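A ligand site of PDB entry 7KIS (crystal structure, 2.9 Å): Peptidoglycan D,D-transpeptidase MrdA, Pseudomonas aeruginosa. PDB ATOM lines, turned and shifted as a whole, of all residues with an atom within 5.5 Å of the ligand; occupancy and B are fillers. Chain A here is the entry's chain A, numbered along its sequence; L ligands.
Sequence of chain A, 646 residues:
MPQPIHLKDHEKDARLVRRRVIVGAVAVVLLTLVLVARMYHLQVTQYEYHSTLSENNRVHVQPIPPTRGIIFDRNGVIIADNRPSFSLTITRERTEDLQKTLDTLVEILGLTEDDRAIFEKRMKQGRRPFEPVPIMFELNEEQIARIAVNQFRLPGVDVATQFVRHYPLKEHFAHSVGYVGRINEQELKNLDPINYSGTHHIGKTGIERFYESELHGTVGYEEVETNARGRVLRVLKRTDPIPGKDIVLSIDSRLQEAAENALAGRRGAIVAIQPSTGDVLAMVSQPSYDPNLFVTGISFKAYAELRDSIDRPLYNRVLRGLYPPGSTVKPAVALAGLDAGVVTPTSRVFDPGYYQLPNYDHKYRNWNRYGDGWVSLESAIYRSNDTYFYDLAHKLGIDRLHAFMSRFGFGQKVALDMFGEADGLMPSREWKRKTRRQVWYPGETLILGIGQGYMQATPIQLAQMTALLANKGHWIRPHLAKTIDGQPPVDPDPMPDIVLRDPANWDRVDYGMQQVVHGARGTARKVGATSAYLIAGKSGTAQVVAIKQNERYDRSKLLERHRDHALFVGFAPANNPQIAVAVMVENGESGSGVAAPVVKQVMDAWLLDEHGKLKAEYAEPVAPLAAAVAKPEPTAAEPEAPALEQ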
ATOM      1  N   GLY A 326       0.944 -17.901 -17.835  1.00  0.00           N
ATOM      2  CA  GLY A 326       2.205 -18.179 -18.486  1.00  0.00           C
ATOM      3  C   GLY A 326       2.034 -18.813 -19.855  1.00  0.00           C
ATOM      4  O   GLY A 326       1.088 -18.528 -20.591  1.00  0.00           O
ATOM      5  N   SER A 327       2.973 -19.695 -20.191  1.00  0.00           N
ATOM      6  CA  SER A 327       3.000 -20.330 -21.492  1.00  0.00           C
ATOM      7  C   SER A 327       1.837 -21.288 -21.710  1.00  0.00           C
ATOM      8  O   SER A 327       1.611 -21.715 -22.853  1.00  0.00           O
ATOM      9  CB  SER A 327       4.315 -21.083 -21.685  1.00  0.00           C
ATOM     10  OG  SER A 327       5.434 -20.211 -21.561  1.00  0.00           O
ATOM     11  N   THR A 328       1.087 -21.637 -20.664  1.00  0.00           N
ATOM     12  CA  THR A 328       0.007 -22.600 -20.802  1.00  0.00           C
ATOM     13  C   THR A 328      -1.107 -22.105 -21.720  1.00  0.00           C
ATOM     14  O   THR A 328      -1.834 -22.926 -22.281  1.00  0.00           O
ATOM     15  CB  THR A 328      -0.564 -22.966 -19.430  1.00  0.00           C
ATOM     16  OG1 THR A 328      -1.170 -21.805 -18.836  1.00  0.00           O
ATOM     17  CG2 THR A 328       0.541 -23.471 -18.513  1.00  0.00           C
ATOM     18  N   LYS A 330      -0.756 -20.620 -24.579  1.00  0.00           N
ATOM     19  CA  LYS A 330      -0.341 -20.531 -25.979  1.00  0.00           C
ATOM     20  C   LYS A 330      -1.195 -21.346 -26.945  1.00  0.00           C
ATOM     21  O   LYS A 330      -1.411 -20.867 -28.069  1.00  0.00           O
ATOM     22  CB  LYS A 330       1.141 -20.920 -26.076  1.00  0.00           C
ATOM     23  CG  LYS A 330       2.081 -19.860 -25.547  1.00  0.00           C
ATOM     24  CD  LYS A 330       3.513 -20.356 -25.440  1.00  0.00           C
ATOM     25  CE  LYS A 330       4.436 -19.259 -24.931  1.00  0.00           C
ATOM     26  NZ  LYS A 330       5.865 -19.545 -25.240  1.00  0.00           N
ATOM     27  N   ARG A 365      12.400 -10.724 -25.840  1.00  0.00           N
ATOM     28  CA  ARG A 365      13.329 -11.829 -25.997  1.00  0.00           C
ATOM     29  C   ARG A 365      12.674 -13.174 -25.741  1.00  0.00           C
ATOM     30  O   ARG A 365      11.737 -13.298 -24.942  1.00  0.00           O
ATOM     31  CB  ARG A 365      14.527 -11.635 -25.071  1.00  0.00           C
ATOM     32  CG  ARG A 365      15.207 -10.297 -25.291  1.00  0.00           C
ATOM     33  CD  ARG A 365      16.445 -10.115 -24.424  1.00  0.00           C
ATOM     34  NE  ARG A 365      17.284  -9.042 -24.936  1.00  0.00           N
ATOM     35  CZ  ARG A 365      18.143  -9.190 -25.941  1.00  0.00           C
ATOM     36  NH1 ARG A 365      18.873  -8.153 -26.349  1.00  0.00           N
ATOM     37  NH2 ARG A 365      18.291 -10.362 -26.531  1.00  0.00           N
ATOM     38  N   ASN A 366      13.162 -14.192 -26.438  1.00  0.00           N
ATOM     39  CA  ASN A 366      12.692 -15.557 -26.292  1.00  0.00           C
ATOM     40  C   ASN A 366      13.345 -16.211 -25.079  1.00  0.00           C
ATOM     41  O   ASN A 366      14.419 -15.818 -24.641  1.00  0.00           O
ATOM     42  CB  ASN A 366      13.003 -16.359 -27.570  1.00  0.00           C
ATOM     43  CG  ASN A 366      12.174 -17.631 -27.683  1.00  0.00           C
ATOM     44  OD1 ASN A 366      11.025 -17.687 -27.251  1.00  0.00           O
ATOM     45  ND2 ASN A 366      12.768 -18.657 -28.281  1.00  0.00           N
ATOM     46  N   TRP A 367      12.671 -17.234 -24.539  1.00  0.00           N
ATOM     47  CA  TRP A 367      13.249 -17.956 -23.412  1.00  0.00           C
ATOM     48  C   TRP A 367      14.537 -18.678 -23.797  1.00  0.00           C
ATOM     49  O   TRP A 367      15.378 -18.929 -22.926  1.00  0.00           O
ATOM     50  CB  TRP A 367      12.241 -18.970 -22.842  1.00  0.00           C
ATOM     51  CG  TRP A 367      12.061 -20.210 -23.670  1.00  0.00           C
ATOM     52  CD1 TRP A 367      11.116 -20.427 -24.626  1.00  0.00           C
ATOM     53  CD2 TRP A 367      12.852 -21.403 -23.605  1.00  0.00           C
ATOM     54  NE1 TRP A 367      11.271 -21.676 -25.166  1.00  0.00           N
ATOM     55  CE2 TRP A 367      12.334 -22.297 -24.561  1.00  0.00           C
ATOM     56  CE3 TRP A 367      13.963 -21.797 -22.846  1.00  0.00           C
ATOM     57  CZ2 TRP A 367      12.869 -23.572 -24.767  1.00  0.00           C
ATOM     58  CZ3 TRP A 367      14.486 -23.061 -23.055  1.00  0.00           C
ATOM     59  CH2 TRP A 367      13.945 -23.926 -24.003  1.00  0.00           C
ATOM     60  N   ARG A 369      17.741 -17.756 -25.758  1.00  0.00           N
ATOM     61  CA  ARG A 369      18.343 -16.523 -26.253  1.00  0.00           C
ATOM     62  C   ARG A 369      18.772 -16.639 -27.703  1.00  0.00           C
ATOM     63  O   ARG A 369      18.689 -15.659 -28.462  1.00  0.00           O
ATOM     64  CB  ARG A 369      19.523 -16.121 -25.365  1.00  0.00           C
ATOM     65  CG  ARG A 369      19.195 -14.994 -24.387  1.00  0.00           C
ATOM     66  CD  ARG A 369      17.844 -15.223 -23.718  1.00  0.00           C
ATOM     67  NE  ARG A 369      17.484 -14.158 -22.783  1.00  0.00           N
ATOM     68  CZ  ARG A 369      16.416 -14.194 -21.997  1.00  0.00           C
ATOM     69  NH1 ARG A 369      15.597 -15.236 -22.028  1.00  0.00           N
ATOM     70  NH2 ARG A 369      16.154 -13.177 -21.181  1.00  0.00           N
ATOM     71  N   SER A 384       7.365 -24.200 -27.134  1.00  0.00           N
ATOM     72  CA  SER A 384       6.863 -22.984 -26.494  1.00  0.00           C
ATOM     73  C   SER A 384       7.748 -21.778 -26.840  1.00  0.00           C
ATOM     74  O   SER A 384       8.363 -21.149 -25.989  1.00  0.00           O
ATOM     75  CB  SER A 384       6.771 -23.170 -24.985  1.00  0.00           C
ATOM     76  OG  SER A 384       6.144 -22.048 -24.384  1.00  0.00           O
ATOM     77  N   ASP A 386       8.437 -18.017 -27.759  1.00  0.00           N
ATOM     78  CA  ASP A 386       7.762 -16.784 -27.399  1.00  0.00           C
ATOM     79  C   ASP A 386       7.615 -15.841 -28.589  1.00  0.00           C
ATOM     80  O   ASP A 386       6.617 -15.123 -28.688  1.00  0.00           O
ATOM     81  CB  ASP A 386       8.497 -16.079 -26.251  1.00  0.00           C
ATOM     82  CG  ASP A 386       8.561 -16.926 -25.001  1.00  0.00           C
ATOM     83  OD1 ASP A 386       7.521 -17.499 -24.614  1.00  0.00           O
ATOM     84  OD2 ASP A 386       9.653 -17.026 -24.399  1.00  0.00           O
ATOM     85  N   TYR A 390       4.605 -13.763 -29.701  1.00  0.00           N
ATOM     86  CA  TYR A 390       4.818 -12.326 -29.808  1.00  0.00           C
ATOM     87  C   TYR A 390       4.297 -11.806 -31.147  1.00  0.00           C
ATOM     88  O   TYR A 390       3.570 -10.820 -31.209  1.00  0.00           O
ATOM     89  CB  TYR A 390       6.306 -11.998 -29.654  1.00  0.00           C
ATOM     90  CG  TYR A 390       6.855 -12.096 -28.248  1.00  0.00           C
ATOM     91  CD1 TYR A 390       6.044 -11.878 -27.136  1.00  0.00           C
ATOM     92  CD2 TYR A 390       8.192 -12.395 -28.037  1.00  0.00           C
ATOM     93  CE1 TYR A 390       6.555 -11.969 -25.860  1.00  0.00           C
ATOM     94  CE2 TYR A 390       8.711 -12.484 -26.756  1.00  0.00           C
ATOM     95  CZ  TYR A 390       7.896 -12.269 -25.674  1.00  0.00           C
ATOM     96  OH  TYR A 390       8.412 -12.364 -24.405  1.00  0.00           O
ATOM     97  N   ILE A 450       1.959 -14.651 -24.726  1.00  0.00           N
ATOM     98  CA  ILE A 450       2.600 -15.752 -24.010  1.00  0.00           C
ATOM     99  C   ILE A 450       2.067 -15.843 -22.575  1.00  0.00           C
ATOM    100  O   ILE A 450       2.687 -16.484 -21.727  1.00  0.00           O
ATOM    101  CB  ILE A 450       4.127 -15.630 -24.038  1.00  0.00           C
ATOM    102  CG1 ILE A 450       4.594 -14.367 -23.324  1.00  0.00           C
ATOM    103  CG2 ILE A 450       4.631 -15.652 -25.485  1.00  0.00           C
ATOM    104  CD1 ILE A 450       6.094 -14.306 -23.142  1.00  0.00           C
ATOM    105  N   GLN A 452       1.184 -13.314 -20.093  1.00  0.00           N
ATOM    106  CA  GLN A 452       1.747 -12.499 -19.015  1.00  0.00           C
ATOM    107  C   GLN A 452       1.023 -11.164 -18.890  1.00  0.00           C
ATOM    108  O   GLN A 452      -0.158 -11.055 -19.245  1.00  0.00           O
ATOM    109  CB  GLN A 452       3.238 -12.270 -19.244  1.00  0.00           C
ATOM    110  CG  GLN A 452       4.109 -13.255 -18.489  1.00  0.00           C
ATOM    111  CD  GLN A 452       5.285 -13.745 -19.316  1.00  0.00           C
ATOM    112  OE1 GLN A 452       5.718 -13.070 -20.254  1.00  0.00           O
ATOM    113  NE2 GLN A 452       5.806 -14.914 -18.971  1.00  0.00           N
ATOM    114  N   THR A 523       9.177 -30.083 -24.675  1.00  0.00           N
ATOM    115  CA  THR A 523       9.694 -29.633 -23.392  1.00  0.00           C
ATOM    116  C   THR A 523       9.539 -30.714 -22.326  1.00  0.00           C
ATOM    117  O   THR A 523      10.389 -30.843 -21.434  1.00  0.00           O
ATOM    118  CB  THR A 523       8.996 -28.348 -22.955  1.00  0.00           C
ATOM    119  OG1 THR A 523       7.588 -28.570 -22.875  1.00  0.00           O
ATOM    120  CG2 THR A 523       9.275 -27.230 -23.963  1.00  0.00           C
ATOM    121  N   LYS A 538       0.664 -29.086 -22.106  1.00  0.00           N
ATOM    122  CA  LYS A 538       1.643 -28.023 -22.311  1.00  0.00           C
ATOM    123  C   LYS A 538       2.071 -27.481 -20.955  1.00  0.00           C
ATOM    124  O   LYS A 538       1.222 -27.206 -20.100  1.00  0.00           O
ATOM    125  CB  LYS A 538       1.096 -26.888 -23.183  1.00  0.00           C
ATOM    126  CG  LYS A 538       2.177 -25.867 -23.494  1.00  0.00           C
ATOM    127  CD  LYS A 538       1.667 -24.737 -24.349  1.00  0.00           C
ATOM    128  CE  LYS A 538       2.833 -23.907 -24.844  1.00  0.00           C
ATOM    129  NZ  LYS A 538       3.800 -23.677 -23.740  1.00  0.00           N
ATOM    130  N   SER A 539       3.372 -27.321 -20.776  1.00  0.00           N
ATOM    131  CA  SER A 539       3.926 -26.795 -19.536  1.00  0.00           C
ATOM    132  C   SER A 539       4.089 -25.288 -19.625  1.00  0.00           C
ATOM    133  O   SER A 539       4.103 -24.693 -20.711  1.00  0.00           O
ATOM    134  CB  SER A 539       5.270 -27.449 -19.225  1.00  0.00           C
ATOM    135  OG  SER A 539       6.032 -27.647 -20.399  1.00  0.00           O
ATOM    136  N   GLY A 540       4.223 -24.669 -18.456  1.00  0.00           N
ATOM    137  CA  GLY A 540       4.467 -23.238 -18.384  1.00  0.00           C
ATOM    138  C   GLY A 540       4.967 -22.865 -17.012  1.00  0.00           C
ATOM    139  O   GLY A 540       5.162 -23.710 -16.134  1.00  0.00           O
ATOM    140  N   THR A 541       5.185 -21.562 -16.843  1.00  0.00           N
ATOM    141  CA  THR A 541       5.643 -20.982 -15.583  1.00  0.00           C
ATOM    142  C   THR A 541       4.774 -19.771 -15.290  1.00  0.00           C
ATOM    143  O   THR A 541       4.370 -19.051 -16.198  1.00  0.00           O
ATOM    144  CB  THR A 541       7.115 -20.593 -15.629  1.00  0.00           C
ATOM    145  OG1 THR A 541       7.352 -19.712 -16.739  1.00  0.00           O
ATOM    146  CG2 THR A 541       8.001 -21.823 -15.774  1.00  0.00           C
ATOM    147  N   GLN A 543       4.378 -16.066 -13.107  1.00  0.00           N
ATOM    148  CA  GLN A 543       5.278 -14.971 -12.768  1.00  0.00           C
ATOM    149  C   GLN A 543       5.170 -14.631 -11.287  1.00  0.00           C
ATOM    150  O   GLN A 543       4.077 -14.597 -10.727  1.00  0.00           O
ATOM    151  CB  GLN A 543       4.958 -13.729 -13.597  1.00  0.00           C
ATOM    152  CG  GLN A 543       4.570 -13.937 -15.063  1.00  0.00           C
ATOM    153  CD  GLN A 543       5.312 -15.066 -15.765  1.00  0.00           C
ATOM    154  OE1 GLN A 543       4.708 -15.848 -16.491  1.00  0.00           O
ATOM    155  NE2 GLN A 543       6.624 -15.134 -15.569  1.00  0.00           N
ATOM    156  N   LEU A 567       3.685 -24.683 -13.935  1.00  0.00           N
ATOM    157  CA  LEU A 567       2.334 -24.981 -14.404  1.00  0.00           C
ATOM    158  C   LEU A 567       2.384 -26.042 -15.495  1.00  0.00           C
ATOM    159  O   LEU A 567       3.318 -26.095 -16.290  1.00  0.00           O
ATOM    160  CB  LEU A 567       1.636 -23.723 -14.951  1.00  0.00           C
ATOM    161  CG  LEU A 567       0.807 -22.873 -13.971  1.00  0.00           C
ATOM    162  CD1 LEU A 567       1.690 -22.233 -12.921  1.00  0.00           C
ATOM    163  CD2 LEU A 567       0.021 -21.820 -14.728  1.00  0.00           C
ATOM    164  N   GLU A 589       9.221 -23.879 -10.343  1.00  0.00           N
ATOM    165  CA  GLU A 589      10.171 -23.471 -11.381  1.00  0.00           C
ATOM    166  C   GLU A 589       9.967 -24.194 -12.709  1.00  0.00           C
ATOM    167  O   GLU A 589       9.649 -23.559 -13.725  1.00  0.00           O
ATOM    168  CB  GLU A 589      11.616 -23.680 -10.918  1.00  0.00           C
ATOM    169  CG  GLU A 589      12.054 -22.738  -9.815  1.00  0.00           C
ATOM    170  CD  GLU A 589      12.762 -21.492 -10.349  1.00  0.00           C
ATOM    171  OE1 GLU A 589      13.910 -21.237  -9.925  1.00  0.00           O
ATOM    172  OE2 GLU A 589      12.184 -20.785 -11.189  1.00  0.00           O
ATOM    173  N   SER A 590      10.168 -25.502 -12.722  1.00  0.00           N
ATOM    174  CA  SER A 590      10.155 -26.267 -13.978  1.00  0.00           C
ATOM    175  C   SER A 590       8.755 -26.785 -14.246  1.00  0.00           C
ATOM    176  O   SER A 590       8.330 -27.785 -13.668  1.00  0.00           O
ATOM    177  CB  SER A 590      11.159 -27.412 -13.902  1.00  0.00           C
ATOM    178  OG  SER A 590      11.420 -27.973 -15.178  1.00  0.00           O
ATOM    179  N   GLY A 591       8.035 -26.128 -15.151  1.00  0.00           N
ATOM    180  CA  GLY A 591       6.748 -26.667 -15.569  1.00  0.00           C
ATOM    181  C   GLY A 591       6.904 -28.020 -16.228  1.00  0.00           C
ATOM    182  O   GLY A 591       6.058 -28.903 -16.082  1.00  0.00           O
ATOM    183  N   SER A 592       7.990 -28.204 -16.956  1.00  0.00           N
ATOM    184  CA  SER A 592       8.302 -29.469 -17.603  1.00  0.00           C
ATOM    185  C   SER A 592       8.846 -30.534 -16.635  1.00  0.00           C
ATOM    186  O   SER A 592       8.746 -31.721 -16.949  1.00  0.00           O
ATOM    187  CB  SER A 592       9.289 -29.238 -18.718  1.00  0.00           C
ATOM    188  OG  SER A 592      10.417 -28.546 -18.232  1.00  0.00           O
ATOM    189  N   GLY A 593       9.435 -30.134 -15.503  1.00  0.00           N
ATOM    190  CA  GLY A 593      10.143 -31.087 -14.656  1.00  0.00           C
ATOM    191  C   GLY A 593       9.445 -31.492 -13.372  1.00  0.00           C
ATOM    192  O   GLY A 593       9.713 -32.588 -12.846  1.00  0.00           O
HETATM  193  O1  LIG L   1       8.133 -26.246 -18.725  1.00  0.00           O
HETATM  194  S1  LIG L   1       8.933 -25.161 -19.426  1.00  0.00           S
HETATM  195  O2  LIG L   1      10.091 -24.709 -18.556  1.00  0.00           O
HETATM  196  O3  LIG L   1       9.422 -25.896 -20.663  1.00  0.00           O
HETATM  197  O4  LIG L   1       7.950 -23.842 -19.850  1.00  0.00           O
HETATM  198  N1  LIG L   1       8.401 -23.343 -21.115  1.00  0.00           N
HETATM  199  C1  LIG L   1       9.004 -21.953 -20.952  1.00  0.00           C
HETATM  200  C2  LIG L   1       9.185 -21.675 -19.506  1.00  0.00           C
HETATM  201  C3  LIG L   1       9.600 -20.288 -19.236  1.00  0.00           C
HETATM  202  C4  LIG L   1       8.132 -20.924 -21.663  1.00  0.00           C
HETATM  203  N2  LIG L   1       7.629 -19.825 -20.761  1.00  0.00           N
HETATM  204  C5  LIG L   1       6.189 -19.701 -20.533  1.00  0.00           C
HETATM  205  O5  LIG L   1       5.783 -19.333 -19.476  1.00  0.00           O
HETATM  206  C6  LIG L   1       8.562 -19.277 -19.703  1.00  0.00           C
HETATM  207  C7  LIG L   1       9.295 -18.053 -20.231  1.00  0.00           C
HETATM  208  O6  LIG L   1      10.119 -17.545 -19.553  1.00  0.00           O
HETATM  209  N3  LIG L   1       9.017 -17.509 -21.579  1.00  0.00           N
HETATM  210  N4  LIG L   1       9.759 -16.371 -21.982  1.00  0.00           N
HETATM  211  C8  LIG L   1       9.618 -15.101 -21.263  1.00  0.00           C
HETATM  212  O7  LIG L   1       8.873 -15.018 -20.341  1.00  0.00           O
HETATM  213  C9  LIG L   1      10.475 -13.862 -21.707  1.00  0.00           C
HETATM  214  C10 LIG L   1      11.946 -14.351 -21.962  1.00  0.00           C
HETATM  215  C11 LIG L   1      12.783 -13.818 -20.733  1.00  0.00           C
HETATM  216  N5  LIG L   1      12.121 -12.715 -20.314  1.00  0.00           N
HETATM  217  C12 LIG L   1      10.531 -12.974 -20.670  1.00  0.00           C
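An oxygen (O5) of the ligand is in hydrogen-bond range of the backbone NH (N) of Ser 327, at 2.9 Å. The side-chain hydroxyl (OG) of Ser 327 is bonded to a carbon (C5) of the ligand (1.4 Å). The side-chain hydroxyl of Ser 539 is in hydrogen-bond range of an oxygen (O1) of the ligand, 3.0 Å away. A nitrogen (N4) of the ligand sits at hydrogen-bond distance from the side-chain carboxylate (OD2) of Asp 386. An oxygen (O7) of the ligand is in hydrogen-bond range of the side-chain amide nitrogen (NE2) of Gln 452 (3.4 Å). OG1 of Thr 541 lies within hydrogen-bond range of O5 of the ligand (3.2 Å). The backbone NH (N) of Ser 592 sits at hydrogen-bond distance from an oxygen (O1) of the ligand (2.6 Å). The side-chain hydroxyl (OG) of Ser 592 sits close to an oxygen (O1) of the ligand (3.3 Å).
OG of Ser 592 sits at hydrogen-bond distance from OG of Ser 590, 3.3 Å away. The side-chain hydroxyl of Ser 327 lies close to the side-chain hydroxyl of Ser 384. The side-chain amide oxygen of Gln 543 lies within hydrogen-bond range of the side-chain amide nitrogen of Gln 452, at 2.9 Å. O of Ser 384 is in hydrogen-bond range of NE1 of Trp 367, at 3.1 Å. OG of Ser 384 is in hydrogen-bond range of NZ of Lys 538, 2.9 Å away. NH1 of Arg 369 sits at hydrogen-bond distance from O of Asn 366 (2.9 Å). The side-chain amino group of Lys 538 lies within hydrogen-bond range of the backbone carbonyl oxygen of Ser 327 (3.1 Å). O of Arg 365 lies within hydrogen-bond range of OH of Tyr 390 (3.5 Å).
Gly 326 touches the ligand (C to O5, 3.8 Å). Arg 365 touches the ligand. Asn 366 touches the ligand (C to C10, 3.9 Å). Trp 367 touches the ligand (CB to N4, 3.7 Å). Arg 369 touches the ligand (NH1 to C11, 3.4 Å). OG of Ser 384 touches C4 of the ligand (3.6 Å). OH of Tyr 390 touches C9 of the ligand, 3.7 Å away. CB of Thr 523 touches O3 of the ligand (3.4 Å). CA of Gly 540 touches O4 of the ligand (3.8 Å). Gly 591 touches the ligand (C to O1, 3.3 Å). Hydrophobic or aromatic side chains that line the ligand: Trp 367. Within 4 Å of the ligand: Gly 326, Ser 327, Arg 365, Asn 366, Trp 367, Arg 369, Ser 384, Asp 386, Tyr 390, Gln 452, Thr 523, Ser 539, Gly 540, Thr 541, Gly 591 and Ser 592. Along chain A the residues within 4 Å of the ligand span positions 326 to 592.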
